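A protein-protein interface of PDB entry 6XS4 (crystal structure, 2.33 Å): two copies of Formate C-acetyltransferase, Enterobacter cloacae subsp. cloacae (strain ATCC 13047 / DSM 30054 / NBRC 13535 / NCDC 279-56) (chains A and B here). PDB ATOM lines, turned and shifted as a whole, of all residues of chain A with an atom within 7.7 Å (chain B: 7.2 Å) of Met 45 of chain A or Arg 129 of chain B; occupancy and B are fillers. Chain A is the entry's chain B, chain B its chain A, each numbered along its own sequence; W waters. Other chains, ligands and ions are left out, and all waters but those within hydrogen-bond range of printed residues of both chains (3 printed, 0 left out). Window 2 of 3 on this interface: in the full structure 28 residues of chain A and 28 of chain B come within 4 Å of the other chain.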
ATOM      1  N   GLU A  39      18.136 -21.587   6.179  1.00  0.00           N
ATOM      2  CA  GLU A  39      16.923 -21.722   5.380  1.00  0.00           C
ATOM      3  C   GLU A  39      15.762 -20.956   6.003  1.00  0.00           C
ATOM      4  O   GLU A  39      15.029 -20.241   5.309  1.00  0.00           O
ATOM      5  CB  GLU A  39      16.569 -23.201   5.220  1.00  0.00           C
ATOM      6  CG  GLU A  39      17.523 -23.969   4.322  1.00  0.00           C
ATOM      7  CD  GLU A  39      17.248 -25.455   4.318  1.00  0.00           C
ATOM      8  OE1 GLU A  39      16.430 -25.911   5.142  1.00  0.00           O
ATOM      9  OE2 GLU A  39      17.852 -26.167   3.488  1.00  0.00           O
ATOM     10  N   MET A  40      15.576 -21.093   7.317  1.00  0.00           N
ATOM     11  CA  MET A  40      14.444 -20.442   7.966  1.00  0.00           C
ATOM     12  C   MET A  40      14.683 -18.948   8.146  1.00  0.00           C
ATOM     13  O   MET A  40      13.755 -18.148   7.975  1.00  0.00           O
ATOM     14  CB  MET A  40      14.156 -21.106   9.313  1.00  0.00           C
ATOM     15  CG  MET A  40      13.583 -22.516   9.201  1.00  0.00           C
ATOM     16  SD  MET A  40      12.031 -22.599   8.280  1.00  0.00           S
ATOM     17  CE  MET A  40      12.594 -23.294   6.729  1.00  0.00           C
ATOM     18  N   TYR A  41      15.911 -18.551   8.491  1.00  0.00           N
ATOM     19  CA  TYR A  41      16.231 -17.128   8.538  1.00  0.00           C
ATOM     20  C   TYR A  41      15.944 -16.454   7.203  1.00  0.00           C
ATOM     21  O   TYR A  41      15.542 -15.286   7.170  1.00  0.00           O
ATOM     22  CB  TYR A  41      17.698 -16.927   8.917  1.00  0.00           C
ATOM     23  CG  TYR A  41      17.926 -16.627  10.382  1.00  0.00           C
ATOM     24  CD1 TYR A  41      17.765 -17.612  11.348  1.00  0.00           C
ATOM     25  CD2 TYR A  41      18.319 -15.362  10.795  1.00  0.00           C
ATOM     26  CE1 TYR A  41      17.981 -17.341  12.689  1.00  0.00           C
ATOM     27  CE2 TYR A  41      18.537 -15.081  12.131  1.00  0.00           C
ATOM     28  CZ  TYR A  41      18.367 -16.074  13.075  1.00  0.00           C
ATOM     29  OH  TYR A  41      18.583 -15.798  14.406  1.00  0.00           O
ATOM     30  N   GLN A  42      16.138 -17.174   6.099  1.00  0.00           N
ATOM     31  CA  GLN A  42      15.892 -16.603   4.782  1.00  0.00           C
ATOM     32  C   GLN A  42      14.413 -16.629   4.415  1.00  0.00           C
ATOM     33  O   GLN A  42      13.934 -15.713   3.737  1.00  0.00           O
ATOM     34  CB  GLN A  42      16.717 -17.352   3.733  1.00  0.00           C
ATOM     35  CG  GLN A  42      18.210 -17.066   3.819  1.00  0.00           C
ATOM     36  CD  GLN A  42      19.042 -18.002   2.960  1.00  0.00           C
ATOM     37  OE1 GLN A  42      18.579 -19.064   2.545  1.00  0.00           O
ATOM     38  NE2 GLN A  42      20.282 -17.607   2.691  1.00  0.00           N
ATOM     39  N   GLN A  43      13.679 -17.653   4.857  1.00  0.00           N
ATOM     40  CA  GLN A  43      12.261 -17.756   4.547  1.00  0.00           C
ATOM     41  C   GLN A  43      11.385 -16.910   5.461  1.00  0.00           C
ATOM     42  O   GLN A  43      10.217 -16.680   5.133  1.00  0.00           O
ATOM     43  CB  GLN A  43      11.794 -19.210   4.648  1.00  0.00           C
ATOM     44  CG  GLN A  43      12.295 -20.126   3.553  1.00  0.00           C
ATOM     45  CD  GLN A  43      11.698 -21.518   3.660  1.00  0.00           C
ATOM     46  OE1 GLN A  43      10.612 -21.699   4.212  1.00  0.00           O
ATOM     47  NE2 GLN A  43      12.411 -22.511   3.138  1.00  0.00           N
ATOM     48  N   HIS A  44      11.910 -16.456   6.600  1.00  0.00           N
ATOM     49  CA  HIS A  44      11.099 -15.788   7.610  1.00  0.00           C
ATOM     50  C   HIS A  44      11.729 -14.476   8.062  1.00  0.00           C
ATOM     51  O   HIS A  44      11.587 -14.080   9.221  1.00  0.00           O
ATOM     52  CB  HIS A  44      10.866 -16.711   8.807  1.00  0.00           C
ATOM     53  CG  HIS A  44      10.043 -17.919   8.482  1.00  0.00           C
ATOM     54  ND1 HIS A  44       8.695 -17.844   8.205  1.00  0.00           N
ATOM     55  CD2 HIS A  44      10.376 -19.227   8.383  1.00  0.00           C
ATOM     56  CE1 HIS A  44       8.232 -19.056   7.951  1.00  0.00           C
ATOM     57  NE2 HIS A  44       9.232 -19.914   8.054  1.00  0.00           N
ATOM     58  N   MET A  45      12.422 -13.784   7.154  1.00  0.00           N
ATOM     59  CA  MET A  45      12.909 -12.445   7.465  1.00  0.00           C
ATOM     60  C   MET A  45      11.782 -11.519   7.898  1.00  0.00           C
ATOM     61  O   MET A  45      12.037 -10.532   8.598  1.00  0.00           O
ATOM     62  CB  MET A  45      13.627 -11.847   6.255  1.00  0.00           C
ATOM     63  CG  MET A  45      15.084 -12.252   6.135  1.00  0.00           C
ATOM     64  SD  MET A  45      15.948 -11.390   4.808  1.00  0.00           S
ATOM     65  CE  MET A  45      15.113 -12.050   3.369  1.00  0.00           C
ATOM     66  N   ASP A  46      10.542 -11.816   7.497  1.00  0.00           N
ATOM     67  CA  ASP A  46       9.400 -10.987   7.854  1.00  0.00           C
ATOM     68  C   ASP A  46       8.919 -11.224   9.278  1.00  0.00           C
ATOM     69  O   ASP A  46       8.181 -10.389   9.815  1.00  0.00           O
ATOM     70  CB  ASP A  46       8.243 -11.245   6.883  1.00  0.00           C
ATOM     71  CG  ASP A  46       7.781 -12.690   6.897  1.00  0.00           C
ATOM     72  OD1 ASP A  46       8.637 -13.591   7.008  1.00  0.00           O
ATOM     73  OD2 ASP A  46       6.558 -12.926   6.801  1.00  0.00           O
ATOM     74  N   LYS A  47       9.302 -12.338   9.897  1.00  0.00           N
ATOM     75  CA  LYS A  47       8.883 -12.605  11.264  1.00  0.00           C
ATOM     76  C   LYS A  47       9.795 -11.881  12.251  1.00  0.00           C
ATOM     77  O   LYS A  47      10.958 -11.607  11.944  1.00  0.00           O
ATOM     78  CB  LYS A  47       8.919 -14.102  11.555  1.00  0.00           C
ATOM     79  CG  LYS A  47       8.238 -14.967  10.511  1.00  0.00           C
ATOM     80  CD  LYS A  47       6.780 -14.583  10.310  1.00  0.00           C
ATOM     81  CE  LYS A  47       6.077 -15.572   9.390  1.00  0.00           C
ATOM     82  NZ  LYS A  47       6.697 -15.628   8.034  1.00  0.00           N
ATOM     83  N   PRO A  48       9.294 -11.557  13.443  1.00  0.00           N
ATOM     84  CA  PRO A  48      10.186 -11.053  14.492  1.00  0.00           C
ATOM     85  C   PRO A  48      11.269 -12.072  14.815  1.00  0.00           C
ATOM     86  O   PRO A  48      11.061 -13.284  14.718  1.00  0.00           O
ATOM     87  CB  PRO A  48       9.249 -10.828  15.684  1.00  0.00           C
ATOM     88  CG  PRO A  48       7.899 -10.663  15.082  1.00  0.00           C
ATOM     89  CD  PRO A  48       7.884 -11.555  13.872  1.00  0.00           C
ATOM     90  N   ILE A  49      12.438 -11.564  15.205  1.00  0.00           N
ATOM     91  CA  ILE A  49      13.584 -12.444  15.428  1.00  0.00           C
ATOM     92  C   ILE A  49      13.240 -13.617  16.337  1.00  0.00           C
ATOM     93  O   ILE A  49      13.585 -14.756  15.993  1.00  0.00           O
ATOM     94  CB  ILE A  49      14.787 -11.620  15.947  1.00  0.00           C
ATOM     95  CG1 ILE A  49      15.251 -10.647  14.860  1.00  0.00           C
ATOM     96  CG2 ILE A  49      15.915 -12.550  16.365  1.00  0.00           C
ATOM     97  CD1 ILE A  49      16.267  -9.621  15.335  1.00  0.00           C
ATOM     98  N   ARG A  52      11.258 -15.998  14.261  1.00  0.00           N
ATOM     99  CA  ARG A  52      12.174 -16.524  13.253  1.00  0.00           C
ATOM    100  C   ARG A  52      13.069 -17.611  13.836  1.00  0.00           C
ATOM    101  O   ARG A  52      13.264 -18.666  13.219  1.00  0.00           O
ATOM    102  CB  ARG A  52      13.014 -15.377  12.688  1.00  0.00           C
ATOM    103  CG  ARG A  52      13.729 -15.670  11.380  1.00  0.00           C
ATOM    104  CD  ARG A  52      14.612 -14.489  10.982  1.00  0.00           C
ATOM    105  NE  ARG A  52      13.918 -13.211  11.133  1.00  0.00           N
ATOM    106  CZ  ARG A  52      14.523 -12.028  11.205  1.00  0.00           C
ATOM    107  NH1 ARG A  52      15.845 -11.944  11.147  1.00  0.00           N
ATOM    108  NH2 ARG A  52      13.801 -10.926  11.347  1.00  0.00           N
ATOM    109  N   TRP A 127      26.275 -15.306   3.590  1.00  0.00           N
ATOM    110  CA  TRP A 127      24.994 -14.664   3.860  1.00  0.00           C
ATOM    111  C   TRP A 127      24.943 -14.071   5.262  1.00  0.00           C
ATOM    112  O   TRP A 127      24.237 -13.082   5.490  1.00  0.00           O
ATOM    113  CB  TRP A 127      23.856 -15.668   3.672  1.00  0.00           C
ATOM    114  CG  TRP A 127      22.499 -15.054   3.788  1.00  0.00           C
ATOM    115  CD1 TRP A 127      21.794 -14.440   2.797  1.00  0.00           C
ATOM    116  CD2 TRP A 127      21.679 -14.994   4.962  1.00  0.00           C
ATOM    117  NE1 TRP A 127      20.585 -14.001   3.280  1.00  0.00           N
ATOM    118  CE2 TRP A 127      20.490 -14.329   4.605  1.00  0.00           C
ATOM    119  CE3 TRP A 127      21.835 -15.439   6.280  1.00  0.00           C
ATOM    120  CZ2 TRP A 127      19.463 -14.096   5.516  1.00  0.00           C
ATOM    121  CZ3 TRP A 127      20.813 -15.207   7.183  1.00  0.00           C
ATOM    122  CH2 TRP A 127      19.642 -14.541   6.797  1.00  0.00           C
ATOM    123  N   GLN A 131      25.475  -9.837   9.800  1.00  0.00           N
ATOM    124  CA  GLN A 131      24.318 -10.158  10.622  1.00  0.00           C
ATOM    125  C   GLN A 131      24.670 -10.938  11.880  1.00  0.00           C
ATOM    126  O   GLN A 131      23.795 -11.142  12.728  1.00  0.00           O
ATOM    127  CB  GLN A 131      23.300 -10.975   9.817  1.00  0.00           C
ATOM    128  CG  GLN A 131      22.904 -10.378   8.484  1.00  0.00           C
ATOM    129  CD  GLN A 131      21.752 -11.125   7.852  1.00  0.00           C
ATOM    130  OE1 GLN A 131      20.634 -11.107   8.365  1.00  0.00           O
ATOM    131  NE2 GLN A 131      22.022 -11.806   6.744  1.00  0.00           N
ATOM    132  N   PRO B  89      12.415   1.835  -1.115  1.00  0.00           N
ATOM    133  CA  PRO B  89      12.134   0.394  -1.012  1.00  0.00           C
ATOM    134  C   PRO B  89      12.005  -0.135   0.406  1.00  0.00           C
ATOM    135  O   PRO B  89      11.466  -1.237   0.581  1.00  0.00           O
ATOM    136  CB  PRO B  89      13.337  -0.247  -1.722  1.00  0.00           C
ATOM    137  CG  PRO B  89      14.447   0.726  -1.505  1.00  0.00           C
ATOM    138  CD  PRO B  89      13.822   2.100  -1.472  1.00  0.00           C
ATOM    139  N   VAL B  93       8.062  -3.016  -1.329  1.00  0.00           N
ATOM    140  CA  VAL B  93       8.275  -3.244  -2.751  1.00  0.00           C
ATOM    141  C   VAL B  93       7.129  -4.018  -3.381  1.00  0.00           C
ATOM    142  O   VAL B  93       7.179  -4.311  -4.579  1.00  0.00           O
ATOM    143  CB  VAL B  93       9.609  -3.974  -3.014  1.00  0.00           C
ATOM    144  CG1 VAL B  93      10.767  -3.198  -2.404  1.00  0.00           C
ATOM    145  CG2 VAL B  93       9.551  -5.404  -2.476  1.00  0.00           C
ATOM    146  N   GLU B  97       6.470  -4.381  -7.453  1.00  0.00           N
ATOM    147  CA  GLU B  97       6.659  -5.573  -8.272  1.00  0.00           C
ATOM    148  C   GLU B  97       5.398  -5.923  -9.053  1.00  0.00           C
ATOM    149  O   GLU B  97       5.487  -6.504 -10.140  1.00  0.00           O
ATOM    150  CB  GLU B  97       7.091  -6.749  -7.393  1.00  0.00           C
ATOM    151  CG  GLU B  97       8.423  -6.521  -6.687  1.00  0.00           C
ATOM    152  CD  GLU B  97       9.041  -7.800  -6.144  1.00  0.00           C
ATOM    153  OE1 GLU B  97       8.400  -8.469  -5.305  1.00  0.00           O
ATOM    154  OE2 GLU B  97      10.170  -8.136  -6.562  1.00  0.00           O
ATOM    155  N   HIS B 122      14.641  -4.270 -10.843  1.00  0.00           N
ATOM    156  CA  HIS B 122      14.642  -5.728 -10.816  1.00  0.00           C
ATOM    157  C   HIS B 122      15.853  -6.275 -10.070  1.00  0.00           C
ATOM    158  O   HIS B 122      15.801  -7.396  -9.555  1.00  0.00           O
ATOM    159  CB  HIS B 122      14.602  -6.294 -12.233  1.00  0.00           C
ATOM    160  CG  HIS B 122      14.403  -7.778 -12.279  1.00  0.00           C
ATOM    161  ND1 HIS B 122      15.333  -8.641 -12.820  1.00  0.00           N
ATOM    162  CD2 HIS B 122      13.385  -8.553 -11.835  1.00  0.00           C
ATOM    163  CE1 HIS B 122      14.893  -9.882 -12.714  1.00  0.00           C
ATOM    164  NE2 HIS B 122      13.713  -9.857 -12.120  1.00  0.00           N
ATOM    165  N   ILE B 124      17.128  -4.470  -7.441  1.00  0.00           N
ATOM    166  CA  ILE B 124      17.017  -3.912  -6.099  1.00  0.00           C
ATOM    167  C   ILE B 124      15.921  -4.608  -5.306  1.00  0.00           C
ATOM    168  O   ILE B 124      16.169  -5.137  -4.216  1.00  0.00           O
ATOM    169  CB  ILE B 124      16.754  -2.391  -6.171  1.00  0.00           C
ATOM    170  CG1 ILE B 124      18.032  -1.655  -6.582  1.00  0.00           C
ATOM    171  CG2 ILE B 124      16.209  -1.876  -4.841  1.00  0.00           C
ATOM    172  CD1 ILE B 124      17.836  -0.175  -6.841  1.00  0.00           C
ATOM    173  N   CYS B 125      14.704  -4.607  -5.845  1.00  0.00           N
ATOM    174  CA  CYS B 125      13.537  -5.057  -5.090  1.00  0.00           C
ATOM    175  C   CYS B 125      13.699  -6.430  -4.453  1.00  0.00           C
ATOM    176  O   CYS B 125      13.391  -6.565  -3.256  1.00  0.00           O
ATOM    177  CB  CYS B 125      12.310  -5.030  -6.013  1.00  0.00           C
ATOM    178  SG  CYS B 125      11.835  -3.364  -6.525  1.00  0.00           S
ATOM    179  N   PRO B 126      14.148  -7.473  -5.156  1.00  0.00           N
ATOM    180  CA  PRO B 126      14.185  -8.801  -4.519  1.00  0.00           C
ATOM    181  C   PRO B 126      15.004  -8.848  -3.238  1.00  0.00           C
ATOM    182  O   PRO B 126      14.667  -9.624  -2.335  1.00  0.00           O
ATOM    183  CB  PRO B 126      14.780  -9.705  -5.612  1.00  0.00           C
ATOM    184  CG  PRO B 126      15.363  -8.785  -6.631  1.00  0.00           C
ATOM    185  CD  PRO B 126      14.571  -7.523  -6.567  1.00  0.00           C
ATOM    186  N   TRP B 127      16.064  -8.044  -3.120  1.00  0.00           N
ATOM    187  CA  TRP B 127      16.849  -8.048  -1.889  1.00  0.00           C
ATOM    188  C   TRP B 127      16.026  -7.572  -0.700  1.00  0.00           C
ATOM    189  O   TRP B 127      16.265  -8.002   0.434  1.00  0.00           O
ATOM    190  CB  TRP B 127      18.094  -7.173  -2.047  1.00  0.00           C
ATOM    191  CG  TRP B 127      18.994  -7.182  -0.839  1.00  0.00           C
ATOM    192  CD1 TRP B 127      20.020  -8.046  -0.591  1.00  0.00           C
ATOM    193  CD2 TRP B 127      18.948  -6.284   0.279  1.00  0.00           C
ATOM    194  NE1 TRP B 127      20.614  -7.744   0.610  1.00  0.00           N
ATOM    195  CE2 TRP B 127      19.975  -6.667   1.165  1.00  0.00           C
ATOM    196  CE3 TRP B 127      18.136  -5.195   0.618  1.00  0.00           C
ATOM    197  CZ2 TRP B 127      20.214  -6.001   2.367  1.00  0.00           C
ATOM    198  CZ3 TRP B 127      18.375  -4.534   1.812  1.00  0.00           C
ATOM    199  CH2 TRP B 127      19.407  -4.940   2.671  1.00  0.00           C
ATOM    200  N   TRP B 128      15.058  -6.687  -0.935  1.00  0.00           N
ATOM    201  CA  TRP B 128      14.265  -6.117   0.146  1.00  0.00           C
ATOM    202  C   TRP B 128      13.112  -7.011   0.583  1.00  0.00           C
ATOM    203  O   TRP B 128      12.504  -6.734   1.622  1.00  0.00           O
ATOM    204  CB  TRP B 128      13.718  -4.750  -0.273  1.00  0.00           C
ATOM    205  CG  TRP B 128      14.745  -3.665  -0.233  1.00  0.00           C
ATOM    206  CD1 TRP B 128      15.519  -3.226  -1.269  1.00  0.00           C
ATOM    207  CD2 TRP B 128      15.118  -2.880   0.906  1.00  0.00           C
ATOM    208  NE1 TRP B 128      16.351  -2.217  -0.844  1.00  0.00           N
ATOM    209  CE2 TRP B 128      16.123  -1.986   0.487  1.00  0.00           C
ATOM    210  CE3 TRP B 128      14.699  -2.848   2.240  1.00  0.00           C
ATOM    211  CZ2 TRP B 128      16.716  -1.070   1.353  1.00  0.00           C
ATOM    212  CZ3 TRP B 128      15.290  -1.936   3.098  1.00  0.00           C
ATOM    213  CH2 TRP B 128      16.285  -1.061   2.652  1.00  0.00           C
ATOM    214  N   ARG B 129      12.795  -8.063  -0.170  1.00  0.00           N
ATOM    215  CA  ARG B 129      11.708  -8.952   0.218  1.00  0.00           C
ATOM    216  C   ARG B 129      11.940  -9.486   1.625  1.00  0.00           C
ATOM    217  O   ARG B 129      13.014 -10.011   1.934  1.00  0.00           O
ATOM    218  CB  ARG B 129      11.585 -10.111  -0.770  1.00  0.00           C
ATOM    219  CG  ARG B 129      11.226  -9.673  -2.175  1.00  0.00           C
ATOM    220  CD  ARG B 129      10.709 -10.829  -3.022  1.00  0.00           C
ATOM    221  NE  ARG B 129      10.604 -10.451  -4.430  1.00  0.00           N
ATOM    222  CZ  ARG B 129      11.316 -10.984  -5.423  1.00  0.00           C
ATOM    223  NH1 ARG B 129      12.196 -11.952  -5.196  1.00  0.00           N
ATOM    224  NH2 ARG B 129      11.131 -10.549  -6.662  1.00  0.00           N
ATOM    225  N   GLY B 130      10.927  -9.349   2.478  1.00  0.00           N
ATOM    226  CA  GLY B 130      11.005  -9.784   3.850  1.00  0.00           C
ATOM    227  C   GLY B 130      11.440  -8.716   4.835  1.00  0.00           C
ATOM    228  O   GLY B 130      11.084  -8.799   6.015  1.00  0.00           O
ATOM    229  N   GLN B 131      12.186  -7.706   4.378  1.00  0.00           N
ATOM    230  CA  GLN B 131      12.738  -6.685   5.256  1.00  0.00           C
ATOM    231  C   GLN B 131      11.939  -5.390   5.265  1.00  0.00           C
ATOM    232  O   GLN B 131      12.231  -4.510   6.082  1.00  0.00           O
ATOM    233  CB  GLN B 131      14.177  -6.353   4.849  1.00  0.00           C
ATOM    234  CG  GLN B 131      15.048  -7.551   4.550  1.00  0.00           C
ATOM    235  CD  GLN B 131      16.506  -7.165   4.419  1.00  0.00           C
ATOM    236  OE1 GLN B 131      17.161  -6.835   5.408  1.00  0.00           O
ATOM    237  NE2 GLN B 131      17.020  -7.191   3.195  1.00  0.00           N
ATOM    238  N   THR B 132      10.960  -5.240   4.376  1.00  0.00           N
ATOM    239  CA  THR B 132      10.233  -3.984   4.282  1.00  0.00           C
ATOM    240  C   THR B 132       9.267  -3.838   5.454  1.00  0.00           C
ATOM    241  O   THR B 132       8.908  -4.807   6.130  1.00  0.00           O
ATOM    242  CB  THR B 132       9.466  -3.896   2.958  1.00  0.00           C
ATOM    243  OG1 THR B 132       8.432  -4.889   2.922  1.00  0.00           O
ATOM    244  CG2 THR B 132      10.409  -4.101   1.776  1.00  0.00           C
ATOM    245  N   ASP B 135       6.062  -5.920   4.736  1.00  0.00           N
ATOM    246  CA  ASP B 135       6.209  -7.363   4.898  1.00  0.00           C
ATOM    247  C   ASP B 135       6.252  -7.753   6.371  1.00  0.00           C
ATOM    248  O   ASP B 135       5.722  -8.801   6.757  1.00  0.00           O
ATOM    249  CB  ASP B 135       7.465  -7.860   4.182  1.00  0.00           C
ATOM    250  CG  ASP B 135       7.257  -8.041   2.692  1.00  0.00           C
ATOM    251  OD1 ASP B 135       8.142  -7.634   1.912  1.00  0.00           O
ATOM    252  OD2 ASP B 135       6.201  -8.582   2.298  1.00  0.00           O
ATOM    253  N   ARG B 136       6.877  -6.924   7.208  1.00  0.00           N
ATOM    254  CA  ARG B 136       6.999  -7.249   8.624  1.00  0.00           C
ATOM    255  C   ARG B 136       5.738  -6.917   9.410  1.00  0.00           C
ATOM    256  O   ARG B 136       5.518  -7.512  10.472  1.00  0.00           O
ATOM    257  CB  ARG B 136       8.211  -6.531   9.219  1.00  0.00           C
ATOM    258  CG  ARG B 136       9.501  -6.938   8.521  1.00  0.00           C
ATOM    259  CD  ARG B 136      10.757  -6.609   9.303  1.00  0.00           C
ATOM    260  NE  ARG B 136      11.773  -7.635   9.068  1.00  0.00           N
ATOM    261  CZ  ARG B 136      13.084  -7.417   9.024  1.00  0.00           C
ATOM    262  NH1 ARG B 136      13.577  -6.197   9.189  1.00  0.00           N
ATOM    263  NH2 ARG B 136      13.906  -8.431   8.799  1.00  0.00           N
HETATM  264  O   HOH W   1       7.560  -8.879  11.888  1.00  0.00           O
HETATM  265  O   HOH W   2       5.100 -11.001   5.615  1.00  0.00           O
HETATM  266  O   HOH W   3      15.369  -8.392  11.498  1.00  0.00           O
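The backbone carbonyl oxygen (O) of Met 45 of chain A lies within hydrogen-bond range of the guanidinium group (NH2) of Arg 136 of chain B, 2.8 Å away. The backbone carbonyl oxygen of Met 45 of chain A sits close to the backbone carbonyl oxygen of Gly 130 of chain B, 3.3 Å away. N of Asp 46 of chain A sits close to O of Gly 130 of chain B, 3.4 Å away.
The side-chain carboxylate (OE2) of Glu 97 of chain B lies within salt-bridge range of the guanidinium group (NH2) of Arg 129 of chain B (2.6 Å). The side-chain amide nitrogen (NE2) of Gln 131 of chain B is in hydrogen-bond range of the backbone carbonyl oxygen (O) of Trp 127 of chain B (3.0 Å). OG1 of Thr 132 of chain B sits at hydrogen-bond distance from OD1 of Asp 135 of chain B, at 2.9 Å. The backbone carbonyl oxygen (O) of His 44 of chain A is in hydrogen-bond range of the guanidinium group (NE) of Arg 52 of chain A (3.1 Å). NH2 of Arg 52 of chain A is in hydrogen-bond range of O of Lys 47 of chain A (3.0 Å). The backbone carbonyl oxygen (O) of Gly 130 of chain B lies within hydrogen-bond range of the guanidinium group (NE) of Arg 136 of chain B (3.3 Å).
Met 45 of chain A touches Arg 129 of chain B (CE to O, 3.3 Å). Gln 131 of chain B touches Met 45 of chain A (CG to SD, 3.95 Å). CB of Asp 46 of chain A touches O of Asp 135 of chain B, at 3.5 Å. O of Asp 46 of chain A touches CA of Arg 136 of chain B, at 3.6 Å. Arg 52 of chain A touches Arg 136 of chain B (NH2 to NH2, 3.6 Å).
Met 45 of chain A touches just these residues of chain B: Arg 129 (3.3 Å), Gly 130 (3.3 Å), Gln 131 (3.95 Å) and Arg 136 (2.8 Å). Of the printed residues of chain B, Asp 46 of chain A touches Gly 130, Asp 135 and Arg 136. Of the printed residues of chain B, Arg 52 of chain A touches Arg 136 (3.6 Å). Of the printed residues of chain A, Gln 131 of chain B touches Met 45 (3.95 Å). Printed residues of chain A within 4 Å of Asp 135 of chain B: Asp 46.
Hydrophobic or aromatic side chains of chain A that line the printed part of chain B: Met 45. Of the 15 printed residues of chain B, 5 touch a printed residue of chain A. Printed residues of chain B that touch a printed residue of chain A: Arg 129, Gly 130, Gln 131, Asp 135 and Arg 136. Among the printed residues, 8 pairs touch across the chains.
Positions printed for both chains: 127 and 131.
Water W2 bridges O of Asp 135 of chain B and OD2 of Asp 46 of chain A. Water W1 lies within hydrogen-bond range of O of Asp 46 of chain A and O of Arg 136 of chain B. Water W3 bridges NH2 of Arg 52 of chain A (3.0 Å) and NH2 of Arg 136 of chain B (3.1 Å).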
